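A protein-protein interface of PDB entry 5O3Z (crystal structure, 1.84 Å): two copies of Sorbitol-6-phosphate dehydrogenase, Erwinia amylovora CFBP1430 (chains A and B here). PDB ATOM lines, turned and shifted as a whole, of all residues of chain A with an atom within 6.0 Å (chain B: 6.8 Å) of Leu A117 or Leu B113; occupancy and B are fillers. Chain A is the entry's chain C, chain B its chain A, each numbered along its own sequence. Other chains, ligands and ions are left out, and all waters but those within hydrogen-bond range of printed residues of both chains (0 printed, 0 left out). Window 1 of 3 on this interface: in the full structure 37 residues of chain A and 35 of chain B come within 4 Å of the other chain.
Printed residues of chain B that touch a printed residue of chain A: Phe B109, Asp B110, Leu B113, Val B118, Ser B156, Ala B160 and Gly B164. Printed residues of chain A that touch a printed residue of chain B: Leu A113, Gln A114, Leu A117, Val A118, Phe A121, Ala A160, Gly A164 and Leu A168. Among the printed residues, no Asp or Glu carboxylate lies within 4 Å of a Lys or Arg side-chain nitrogen of the other chain.
Among the printed residues, pairs that only touch across the chains: Ala A160 with Gly B164 (3.2 Å), Gly A164 with Ala B160 (3.3 Å), Leu A113 with Val B118 (3.4 Å), Phe A121 with Phe B109 (3.5 Å), Val A118 with Asp B110 (3.7 Å), Val A118 with Leu B113 (3.8 Å), Phe A121 with Ser B156 (3.8 Å), Gly A164 with Gly B164 (3.8 Å), Leu A117 with Leu B113 (3.8 Å), Val A118 with Phe B109 (3.8 Å), Leu A168 with Ser B156 (3.9 Å) and Leu A117 with Phe B109 (3.97 Å).
OD1 of Asp B110 sits close to OE1 of Gln A114 (3.2 Å).
Leu A117 touches just these residues of chain B: Phe B109 (3.97 Å) and Leu B113 (3.8 Å). Of the printed residues of chain B, Val A118 touches Phe B109, Asp B110 and Leu B113. Of chain A, only Leu A117 (3.8 Å) and Val A118 (3.8 Å) come within 4 Å of Leu B113. Printed residues of chain A within 4 Å of Val B118: Leu A113. Of the printed residues of chain A, Ser B156 touches Phe A121 (3.8 Å) and Leu A168 (3.9 Å). The nearest printed residue of chain A that does not touch Val B118 is Gln A114 (7.5 Å).
The backbone carbonyl oxygen (O) of Gln A114 sits at hydrogen-bond distance from the backbone NH (N) of Gly A119 (2.9 Å). O of Leu B113 is in hydrogen-bond range of N of Val B118 (2.9 Å). The backbone carbonyl oxygen (O) of Leu A113 is in hydrogen-bond range of the backbone NH (N) of Val A118 (3.0 Å).
Leu A113 touches Val B118, and with the chains exchanged Val A118 touches Leu B113. Leu A117 touches Leu B113, but with the chains exchanged Leu A113 does not touch Leu B117 (4.1 Å). Ala A160 touches Gly B164, and with the chains exchanged Gly A164 touches Ala B160. Gly A164 touches its own counterpart, Gly B164. Positions printed for both chains: 112, 113, 114, 115, 116, 117, 118, 119, 120, 160, 161 and 164. Of the 13 pairs that touch across the chains among the printed residues, 5 have their exchanged pair printed and touching as well.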
ATOM      1  N   TYR A  91       3.700  21.498   0.361  1.00  0.00           N
ATOM      2  CA  TYR A  91       4.397  21.370  -0.857  1.00  0.00           C
ATOM      3  C   TYR A  91       3.992  22.455  -1.793  1.00  0.00           C
ATOM      4  O   TYR A  91       2.904  22.420  -2.373  1.00  0.00           O
ATOM      5  CB  TYR A  91       4.130  19.978  -1.505  1.00  0.00           C
ATOM      6  CG  TYR A  91       5.068  19.751  -2.640  1.00  0.00           C
ATOM      7  CD1 TYR A  91       6.375  19.360  -2.377  1.00  0.00           C
ATOM      8  CD2 TYR A  91       4.706  19.940  -3.962  1.00  0.00           C
ATOM      9  CE1 TYR A  91       7.285  19.227  -3.401  1.00  0.00           C
ATOM     10  CE2 TYR A  91       5.651  19.787  -4.996  1.00  0.00           C
ATOM     11  CZ  TYR A  91       6.930  19.433  -4.677  1.00  0.00           C
ATOM     12  OH  TYR A  91       7.975  19.209  -5.578  1.00  0.00           O
ATOM     13  N   SER A 112       7.830  19.875 -15.632  1.00  0.00           N
ATOM     14  CA  SER A 112       6.530  20.099 -14.942  1.00  0.00           C
ATOM     15  C   SER A 112       6.143  18.906 -14.134  1.00  0.00           C
ATOM     16  O   SER A 112       5.698  19.028 -12.984  1.00  0.00           O
ATOM     17  CB  SER A 112       5.453  20.343 -15.945  1.00  0.00           C
ATOM     18  OG  SER A 112       4.320  20.944 -15.312  1.00  0.00           O
ATOM     19  N   LEU A 113       6.351  17.736 -14.722  1.00  0.00           N
ATOM     20  CA  LEU A 113       6.057  16.490 -14.089  1.00  0.00           C
ATOM     21  C   LEU A 113       6.992  16.229 -12.915  1.00  0.00           C
ATOM     22  O   LEU A 113       6.564  15.737 -11.881  1.00  0.00           O
ATOM     23  CB  LEU A 113       6.203  15.333 -15.120  1.00  0.00           C
ATOM     24  CG  LEU A 113       5.003  14.861 -15.919  1.00  0.00           C
ATOM     25  CD1 LEU A 113       4.012  15.905 -16.321  1.00  0.00           C
ATOM     26  CD2 LEU A 113       5.397  14.010 -17.113  1.00  0.00           C
ATOM     27  N   GLN A 114       8.300  16.492 -13.087  1.00  0.00           N
ATOM     28  CA  GLN A 114       9.220  16.267 -11.995  1.00  0.00           C
ATOM     29  C   GLN A 114       8.940  17.159 -10.738  1.00  0.00           C
ATOM     30  O   GLN A 114       8.903  16.674  -9.600  1.00  0.00           O
ATOM     31  CB  GLN A 114      10.681  16.481 -12.485  1.00  0.00           C
ATOM     32  CG  GLN A 114      11.175  15.463 -13.523  1.00  0.00           C
ATOM     33  CD  GLN A 114      11.101  14.016 -13.087  1.00  0.00           C
ATOM     34  OE1 GLN A 114      10.563  13.152 -13.814  1.00  0.00           O
ATOM     35  NE2 GLN A 114      11.635  13.712 -11.924  1.00  0.00           N
ATOM     36  N   VAL A 115       8.807  18.440 -11.008  1.00  0.00           N
ATOM     37  CA  VAL A 115       8.615  19.489 -10.012  1.00  0.00           C
ATOM     38  C   VAL A 115       7.207  19.408  -9.333  1.00  0.00           C
ATOM     39  O   VAL A 115       7.110  19.569  -8.110  1.00  0.00           O
ATOM     40  CB  VAL A 115       8.878  20.871 -10.621  1.00  0.00           C
ATOM     41  CG1 VAL A 115       8.275  21.975  -9.748  1.00  0.00           C
ATOM     42  CG2 VAL A 115      10.395  21.100 -10.713  1.00  0.00           C
ATOM     43  N   ASN A 116       6.167  19.108 -10.075  1.00  0.00           N
ATOM     44  CA  ASN A 116       4.778  19.100  -9.503  1.00  0.00           C
ATOM     45  C   ASN A 116       4.279  17.775  -9.034  1.00  0.00           C
ATOM     46  O   ASN A 116       3.349  17.705  -8.215  1.00  0.00           O
ATOM     47  CB  ASN A 116       3.807  19.686 -10.526  1.00  0.00           C
ATOM     48  CG  ASN A 116       4.060  21.146 -10.758  1.00  0.00           C
ATOM     49  OD1 ASN A 116       3.986  21.897  -9.826  1.00  0.00           O
ATOM     50  ND2 ASN A 116       4.317  21.566 -12.002  1.00  0.00           N
ATOM     51  N   LEU A 117       4.825  16.695  -9.587  1.00  0.00           N
ATOM     52  CA  LEU A 117       4.367  15.391  -9.245  1.00  0.00           C
ATOM     53  C   LEU A 117       5.419  14.557  -8.541  1.00  0.00           C
ATOM     54  O   LEU A 117       5.180  14.022  -7.469  1.00  0.00           O
ATOM     55  CB  LEU A 117       3.913  14.735 -10.566  1.00  0.00           C
ATOM     56  CG  LEU A 117       2.682  13.922 -10.719  1.00  0.00           C
ATOM     57  CD1 LEU A 117       1.593  14.408  -9.728  1.00  0.00           C
ATOM     58  CD2 LEU A 117       2.214  13.898 -12.172  1.00  0.00           C
ATOM     59  N   VAL A 118       6.593  14.387  -9.149  1.00  0.00           N
ATOM     60  CA  VAL A 118       7.584  13.502  -8.536  1.00  0.00           C
ATOM     61  C   VAL A 118       8.064  14.083  -7.158  1.00  0.00           C
ATOM     62  O   VAL A 118       8.223  13.346  -6.200  1.00  0.00           O
ATOM     63  CB  VAL A 118       8.778  13.217  -9.473  1.00  0.00           C
ATOM     64  CG1 VAL A 118       9.910  12.529  -8.731  1.00  0.00           C
ATOM     65  CG2 VAL A 118       8.401  12.294 -10.636  1.00  0.00           C
ATOM     66  N   GLY A 119       8.314  15.388  -7.088  1.00  0.00           N
ATOM     67  CA  GLY A 119       8.687  16.030  -5.814  1.00  0.00           C
ATOM     68  C   GLY A 119       7.607  15.950  -4.754  1.00  0.00           C
ATOM     69  O   GLY A 119       7.844  15.689  -3.572  1.00  0.00           O
ATOM     70  N   TYR A 120       6.362  16.090  -5.211  1.00  0.00           N
ATOM     71  CA  TYR A 120       5.253  15.945  -4.304  1.00  0.00           C
ATOM     72  C   TYR A 120       5.207  14.528  -3.732  1.00  0.00           C
ATOM     73  O   TYR A 120       4.992  14.318  -2.533  1.00  0.00           O
ATOM     74  CB  TYR A 120       3.978  16.388  -5.022  1.00  0.00           C
ATOM     75  CG  TYR A 120       2.689  16.295  -4.144  1.00  0.00           C
ATOM     76  CD1 TYR A 120       2.723  16.484  -2.778  1.00  0.00           C
ATOM     77  CD2 TYR A 120       1.448  16.136  -4.729  1.00  0.00           C
ATOM     78  CE1 TYR A 120       1.573  16.467  -2.015  1.00  0.00           C
ATOM     79  CE2 TYR A 120       0.255  16.128  -3.968  1.00  0.00           C
ATOM     80  CZ  TYR A 120       0.337  16.234  -2.613  1.00  0.00           C
ATOM     81  OH  TYR A 120      -0.826  16.117  -1.828  1.00  0.00           O
ATOM     82  N   PHE A 121       5.409  13.545  -4.601  1.00  0.00           N
ATOM     83  CA  PHE A 121       5.470  12.116  -4.220  1.00  0.00           C
ATOM     84  C   PHE A 121       6.577  11.790  -3.210  1.00  0.00           C
ATOM     85  O   PHE A 121       6.339  11.176  -2.164  1.00  0.00           O
ATOM     86  CB  PHE A 121       5.567  11.269  -5.501  1.00  0.00           C
ATOM     87  CG  PHE A 121       5.964   9.842  -5.293  1.00  0.00           C
ATOM     88  CD1 PHE A 121       5.015   8.849  -5.030  1.00  0.00           C
ATOM     89  CD2 PHE A 121       7.292   9.457  -5.483  1.00  0.00           C
ATOM     90  CE1 PHE A 121       5.371   7.524  -4.869  1.00  0.00           C
ATOM     91  CE2 PHE A 121       7.658   8.157  -5.286  1.00  0.00           C
ATOM     92  CZ  PHE A 121       6.711   7.196  -4.953  1.00  0.00           C
ATOM     93  N   LEU A 122       7.741  12.340  -3.480  1.00  0.00           N
ATOM     94  CA  LEU A 122       8.925  11.975  -2.707  1.00  0.00           C
ATOM     95  C   LEU A 122       8.809  12.634  -1.336  1.00  0.00           C
ATOM     96  O   LEU A 122       9.035  12.021  -0.315  1.00  0.00           O
ATOM     97  CB  LEU A 122      10.181  12.360  -3.491  1.00  0.00           C
ATOM     98  CG  LEU A 122      10.641  11.457  -4.628  1.00  0.00           C
ATOM     99  CD1 LEU A 122      11.866  12.016  -5.326  1.00  0.00           C
ATOM    100  CD2 LEU A 122      10.889  10.008  -4.222  1.00  0.00           C
ATOM    101  N   ALA A 160      -1.562  19.063 -17.012  1.00  0.00           N
ATOM    102  CA  ALA A 160      -1.265  17.647 -16.840  1.00  0.00           C
ATOM    103  C   ALA A 160      -0.651  17.382 -15.478  1.00  0.00           C
ATOM    104  O   ALA A 160      -1.040  16.420 -14.749  1.00  0.00           O
ATOM    105  CB  ALA A 160      -0.303  17.193 -17.969  1.00  0.00           C
ATOM    106  N   ALA A 161       0.306  18.230 -15.074  1.00  0.00           N
ATOM    107  CA  ALA A 161       0.980  18.065 -13.797  1.00  0.00           C
ATOM    108  C   ALA A 161       0.022  18.348 -12.591  1.00  0.00           C
ATOM    109  O   ALA A 161      -0.005  17.606 -11.586  1.00  0.00           O
ATOM    110  CB  ALA A 161       2.188  19.027 -13.728  1.00  0.00           C
ATOM    111  N   GLY A 164      -2.625  15.820 -12.207  1.00  0.00           N
ATOM    112  CA  GLY A 164      -1.982  14.700 -11.629  1.00  0.00           C
ATOM    113  C   GLY A 164      -1.793  14.780 -10.097  1.00  0.00           C
ATOM    114  O   GLY A 164      -1.875  13.773  -9.391  1.00  0.00           O
ATOM    115  N   GLY A 165      -1.524  15.997  -9.616  1.00  0.00           N
ATOM    116  CA  GLY A 165      -1.438  16.327  -8.222  1.00  0.00           C
ATOM    117  C   GLY A 165      -2.679  15.931  -7.464  1.00  0.00           C
ATOM    118  O   GLY A 165      -2.568  15.360  -6.347  1.00  0.00           O
ATOM    119  N   VAL A 166      -3.839  16.145  -8.114  1.00  0.00           N
ATOM    120  CA  VAL A 166      -5.143  15.839  -7.476  1.00  0.00           C
ATOM    121  C   VAL A 166      -5.236  14.332  -7.316  1.00  0.00           C
ATOM    122  O   VAL A 166      -5.586  13.848  -6.328  1.00  0.00           O
ATOM    123  CB  VAL A 166      -6.303  16.344  -8.290  1.00  0.00           C
ATOM    124  CG1 VAL A 166      -7.603  15.900  -7.755  1.00  0.00           C
ATOM    125  CG2 VAL A 166      -6.285  17.855  -8.408  1.00  0.00           C
ATOM    126  N   LEU A 168      -2.747  12.188  -7.108  1.00  0.00           N
ATOM    127  CA  LEU A 168      -1.823  11.800  -6.069  1.00  0.00           C
ATOM    128  C   LEU A 168      -2.349  12.108  -4.621  1.00  0.00           C
ATOM    129  O   LEU A 168      -2.327  11.239  -3.711  1.00  0.00           O
ATOM    130  CB  LEU A 168      -0.414  12.435  -6.354  1.00  0.00           C
ATOM    131  CG  LEU A 168       0.682  12.131  -5.326  1.00  0.00           C
ATOM    132  CD1 LEU A 168       0.946  10.680  -5.059  1.00  0.00           C
ATOM    133  CD2 LEU A 168       1.972  12.824  -5.722  1.00  0.00           C
ATOM    134  N   THR B  67       7.633   6.388 -25.126  1.00  0.00           N
ATOM    135  CA  THR B  67       8.324   7.194 -24.116  1.00  0.00           C
ATOM    136  C   THR B  67       9.540   7.904 -24.699  1.00  0.00           C
ATOM    137  O   THR B  67      10.108   8.781 -24.050  1.00  0.00           O
ATOM    138  CB  THR B  67       8.810   6.330 -22.918  1.00  0.00           C
ATOM    139  OG1 THR B  67       9.870   5.491 -23.335  1.00  0.00           O
ATOM    140  CG2 THR B  67       7.691   5.433 -22.328  1.00  0.00           C
ATOM    141  N   ASP B 108       9.203   3.167 -10.401  1.00  0.00           N
ATOM    142  CA  ASP B 108       7.839   2.805 -10.871  1.00  0.00           C
ATOM    143  C   ASP B 108       6.970   4.024 -11.058  1.00  0.00           C
ATOM    144  O   ASP B 108       6.197   4.105 -12.019  1.00  0.00           O
ATOM    145  CB  ASP B 108       7.111   1.896  -9.893  1.00  0.00           C
ATOM    146  CG  ASP B 108       7.651   0.485  -9.862  1.00  0.00           C
ATOM    147  OD1 ASP B 108       8.256   0.016 -10.845  1.00  0.00           O
ATOM    148  OD2 ASP B 108       7.458  -0.155  -8.837  1.00  0.00           O
ATOM    149  N   PHE B 109       7.082   4.993 -10.139  1.00  0.00           N
ATOM    150  CA  PHE B 109       6.282   6.196 -10.212  1.00  0.00           C
ATOM    151  C   PHE B 109       6.685   6.905 -11.480  1.00  0.00           C
ATOM    152  O   PHE B 109       5.875   7.319 -12.299  1.00  0.00           O
ATOM    153  CB  PHE B 109       6.564   7.095  -9.014  1.00  0.00           C
ATOM    154  CG  PHE B 109       5.651   8.285  -8.960  1.00  0.00           C
ATOM    155  CD1 PHE B 109       4.387   8.130  -8.436  1.00  0.00           C
ATOM    156  CD2 PHE B 109       6.046   9.507  -9.443  1.00  0.00           C
ATOM    157  CE1 PHE B 109       3.553   9.221  -8.337  1.00  0.00           C
ATOM    158  CE2 PHE B 109       5.198  10.564  -9.423  1.00  0.00           C
ATOM    159  CZ  PHE B 109       3.947  10.413  -8.893  1.00  0.00           C
ATOM    160  N   ASP B 110       7.991   7.023 -11.660  1.00  0.00           N
ATOM    161  CA  ASP B 110       8.529   7.589 -12.882  1.00  0.00           C
ATOM    162  C   ASP B 110       8.100   6.891 -14.172  1.00  0.00           C
ATOM    163  O   ASP B 110       7.753   7.580 -15.142  1.00  0.00           O
ATOM    164  CB  ASP B 110      10.061   7.642 -12.851  1.00  0.00           C
ATOM    165  CG  ASP B 110      10.589   9.003 -12.401  1.00  0.00           C
ATOM    166  OD1 ASP B 110      10.183  10.058 -12.965  1.00  0.00           O
ATOM    167  OD2 ASP B 110      11.421   9.008 -11.474  1.00  0.00           O
ATOM    168  N   LEU B 111       8.189   5.557 -14.192  1.00  0.00           N
ATOM    169  CA  LEU B 111       7.781   4.774 -15.353  1.00  0.00           C
ATOM    170  C   LEU B 111       6.292   5.003 -15.641  1.00  0.00           C
ATOM    171  O   LEU B 111       5.899   5.355 -16.729  1.00  0.00           O
ATOM    172  CB  LEU B 111       8.075   3.296 -15.089  1.00  0.00           C
ATOM    173  CG  LEU B 111       8.009   2.322 -16.287  1.00  0.00           C
ATOM    174  CD1 LEU B 111       8.925   2.706 -17.456  1.00  0.00           C
ATOM    175  CD2 LEU B 111       8.349   0.930 -15.755  1.00  0.00           C
ATOM    176  N   SER B 112       5.469   4.889 -14.611  1.00  0.00           N
ATOM    177  CA  SER B 112       4.037   5.245 -14.796  1.00  0.00           C
ATOM    178  C   SER B 112       3.847   6.559 -15.517  1.00  0.00           C
ATOM    179  O   SER B 112       3.071   6.617 -16.488  1.00  0.00           O
ATOM    180  CB  SER B 112       3.251   5.223 -13.478  1.00  0.00           C
ATOM    181  OG  SER B 112       1.865   5.523 -13.779  1.00  0.00           O
ATOM    182  N   LEU B 113       4.604   7.601 -15.146  1.00  0.00           N
ATOM    183  CA  LEU B 113       4.474   8.905 -15.809  1.00  0.00           C
ATOM    184  C   LEU B 113       4.917   8.870 -17.277  1.00  0.00           C
ATOM    185  O   LEU B 113       4.295   9.479 -18.156  1.00  0.00           O
ATOM    186  CB  LEU B 113       5.235  10.007 -15.062  1.00  0.00           C
ATOM    187  CG  LEU B 113       4.800  10.236 -13.599  1.00  0.00           C
ATOM    188  CD1 LEU B 113       5.597  11.383 -12.989  1.00  0.00           C
ATOM    189  CD2 LEU B 113       3.322  10.497 -13.467  1.00  0.00           C
ATOM    190  N   GLN B 114       5.975   8.122 -17.553  1.00  0.00           N
ATOM    191  CA  GLN B 114       6.511   8.062 -18.927  1.00  0.00           C
ATOM    192  C   GLN B 114       5.488   7.377 -19.871  1.00  0.00           C
ATOM    193  O   GLN B 114       5.107   7.922 -20.876  1.00  0.00           O
ATOM    194  CB  GLN B 114       7.890   7.322 -18.922  1.00  0.00           C
ATOM    195  CG  GLN B 114       9.082   8.145 -18.398  1.00  0.00           C
ATOM    196  CD  GLN B 114       9.255   9.501 -19.104  1.00  0.00           C
ATOM    197  OE1 GLN B 114       9.120   9.607 -20.313  1.00  0.00           O
ATOM    198  NE2 GLN B 114       9.545  10.548 -18.341  1.00  0.00           N
ATOM    199  N   VAL B 115       5.048   6.200 -19.487  1.00  0.00           N
ATOM    200  CA  VAL B 115       4.194   5.339 -20.297  1.00  0.00           C
ATOM    201  C   VAL B 115       2.777   5.954 -20.366  1.00  0.00           C
ATOM    202  O   VAL B 115       2.230   6.107 -21.453  1.00  0.00           O
ATOM    203  CB  VAL B 115       4.188   3.899 -19.759  1.00  0.00           C
ATOM    204  CG1 VAL B 115       3.219   3.016 -20.545  1.00  0.00           C
ATOM    205  CG2 VAL B 115       5.587   3.287 -19.869  1.00  0.00           C
ATOM    206  N   ASN B 116       2.243   6.391 -19.220  1.00  0.00           N
ATOM    207  CA  ASN B 116       0.858   6.827 -19.200  1.00  0.00           C
ATOM    208  C   ASN B 116       0.626   8.225 -19.617  1.00  0.00           C
ATOM    209  O   ASN B 116      -0.474   8.549 -20.068  1.00  0.00           O
ATOM    210  CB  ASN B 116       0.282   6.616 -17.860  1.00  0.00           C
ATOM    211  CG  ASN B 116      -0.004   5.201 -17.625  1.00  0.00           C
ATOM    212  OD1 ASN B 116      -0.826   4.630 -18.373  1.00  0.00           O
ATOM    213  ND2 ASN B 116       0.662   4.580 -16.634  1.00  0.00           N
ATOM    214  N   LEU B 117       1.655   9.068 -19.491  1.00  0.00           N
ATOM    215  CA  LEU B 117       1.486  10.466 -19.665  1.00  0.00           C
ATOM    216  C   LEU B 117       2.386  11.063 -20.692  1.00  0.00           C
ATOM    217  O   LEU B 117       1.899  11.701 -21.584  1.00  0.00           O
ATOM    218  CB  LEU B 117       1.617  11.191 -18.303  1.00  0.00           C
ATOM    219  CG  LEU B 117       1.219  12.644 -18.113  1.00  0.00           C
ATOM    220  CD1 LEU B 117      -0.172  12.877 -18.699  1.00  0.00           C
ATOM    221  CD2 LEU B 117       1.251  12.910 -16.600  1.00  0.00           C
ATOM    222  N   VAL B 118       3.715  10.913 -20.584  1.00  0.00           N
ATOM    223  CA  VAL B 118       4.588  11.556 -21.545  1.00  0.00           C
ATOM    224  C   VAL B 118       4.387  10.946 -22.976  1.00  0.00           C
ATOM    225  O   VAL B 118       4.418  11.653 -23.986  1.00  0.00           O
ATOM    226  CB  VAL B 118       6.059  11.438 -21.097  1.00  0.00           C
ATOM    227  CG1 VAL B 118       7.014  11.762 -22.225  1.00  0.00           C
ATOM    228  CG2 VAL B 118       6.309  12.303 -19.876  1.00  0.00           C
ATOM    229  N   GLY B 119       4.154   9.652 -23.038  1.00  0.00           N
ATOM    230  CA  GLY B 119       3.842   9.007 -24.311  1.00  0.00           C
ATOM    231  C   GLY B 119       2.619   9.603 -24.940  1.00  0.00           C
ATOM    232  O   GLY B 119       2.572   9.803 -26.149  1.00  0.00           O
ATOM    233  N   TYR B 120       1.640   9.948 -24.096  1.00  0.00           N
ATOM    234  CA  TYR B 120       0.404  10.490 -24.601  1.00  0.00           C
ATOM    235  C   TYR B 120       0.636  11.863 -25.138  1.00  0.00           C
ATOM    236  O   TYR B 120       0.105  12.208 -26.182  1.00  0.00           O
ATOM    237  CB  TYR B 120      -0.721  10.383 -23.551  1.00  0.00           C
ATOM    238  CG  TYR B 120      -2.065  11.055 -23.913  1.00  0.00           C
ATOM    239  CD1 TYR B 120      -2.571  11.056 -25.207  1.00  0.00           C
ATOM    240  CD2 TYR B 120      -2.889  11.563 -22.917  1.00  0.00           C
ATOM    241  CE1 TYR B 120      -3.797  11.655 -25.519  1.00  0.00           C
ATOM    242  CE2 TYR B 120      -4.119  12.172 -23.200  1.00  0.00           C
ATOM    243  CZ  TYR B 120      -4.578  12.179 -24.501  1.00  0.00           C
ATOM    244  OH  TYR B 120      -5.770  12.727 -24.816  1.00  0.00           O
ATOM    245  N   SER B 156      -0.732   4.929  -6.279  1.00  0.00           N
ATOM    246  CA  SER B 156      -0.405   6.340  -6.468  1.00  0.00           C
ATOM    247  C   SER B 156       0.163   6.708  -7.831  1.00  0.00           C
ATOM    248  O   SER B 156      -0.217   7.733  -8.407  1.00  0.00           O
ATOM    249  CB  SER B 156       0.481   6.842  -5.308  1.00  0.00           C
ATOM    250  OG  SER B 156       1.807   6.321  -5.383  1.00  0.00           O
ATOM    251  N   GLY B 157       1.099   5.885  -8.340  1.00  0.00           N
ATOM    252  CA  GLY B 157       1.733   6.154  -9.601  1.00  0.00           C
ATOM    253  C   GLY B 157       0.772   6.127 -10.758  1.00  0.00           C
ATOM    254  O   GLY B 157       0.725   7.028 -11.621  1.00  0.00           O
ATOM    255  N   ALA B 160      -1.959   9.222 -10.284  1.00  0.00           N
ATOM    256  CA  ALA B 160      -1.300  10.449 -10.644  1.00  0.00           C
ATOM    257  C   ALA B 160      -1.242  10.607 -12.191  1.00  0.00           C
ATOM    258  O   ALA B 160      -1.575  11.656 -12.768  1.00  0.00           O
ATOM    259  CB  ALA B 160       0.099  10.463 -10.019  1.00  0.00           C
ATOM    260  N   ALA B 161      -0.848   9.528 -12.857  1.00  0.00           N
ATOM    261  CA  ALA B 161      -0.615   9.580 -14.274  1.00  0.00           C
ATOM    262  C   ALA B 161      -1.921   9.590 -15.046  1.00  0.00           C
ATOM    263  O   ALA B 161      -2.005  10.267 -16.001  1.00  0.00           O
ATOM    264  CB  ALA B 161       0.201   8.375 -14.679  1.00  0.00           C
ATOM    265  N   LYS B 162      -2.937   8.838 -14.576  1.00  0.00           N
ATOM    266  CA  LYS B 162      -4.230   8.765 -15.223  1.00  0.00           C
ATOM    267  C   LYS B 162      -5.026  10.024 -15.004  1.00  0.00           C
ATOM    268  O   LYS B 162      -5.590  10.527 -15.934  1.00  0.00           O
ATOM    269  CB  LYS B 162      -5.037   7.548 -14.759  1.00  0.00           C
ATOM    270  CG  LYS B 162      -4.515   6.192 -15.261  1.00  0.00           C
ATOM    271  CD  LYS B 162      -4.403   6.111 -16.782  1.00  0.00           C
ATOM    272  CE  LYS B 162      -3.748   4.796 -17.241  1.00  0.00           C
ATOM    273  NZ  LYS B 162      -3.860   4.606 -18.722  1.00  0.00           N
ATOM    274  N   GLY B 164      -3.547  12.895 -14.582  1.00  0.00           N
ATOM    275  CA  GLY B 164      -2.772  13.772 -15.458  1.00  0.00           C
ATOM    276  C   GLY B 164      -3.166  13.655 -16.911  1.00  0.00           C
ATOM    277  O   GLY B 164      -3.317  14.672 -17.605  1.00  0.00           O
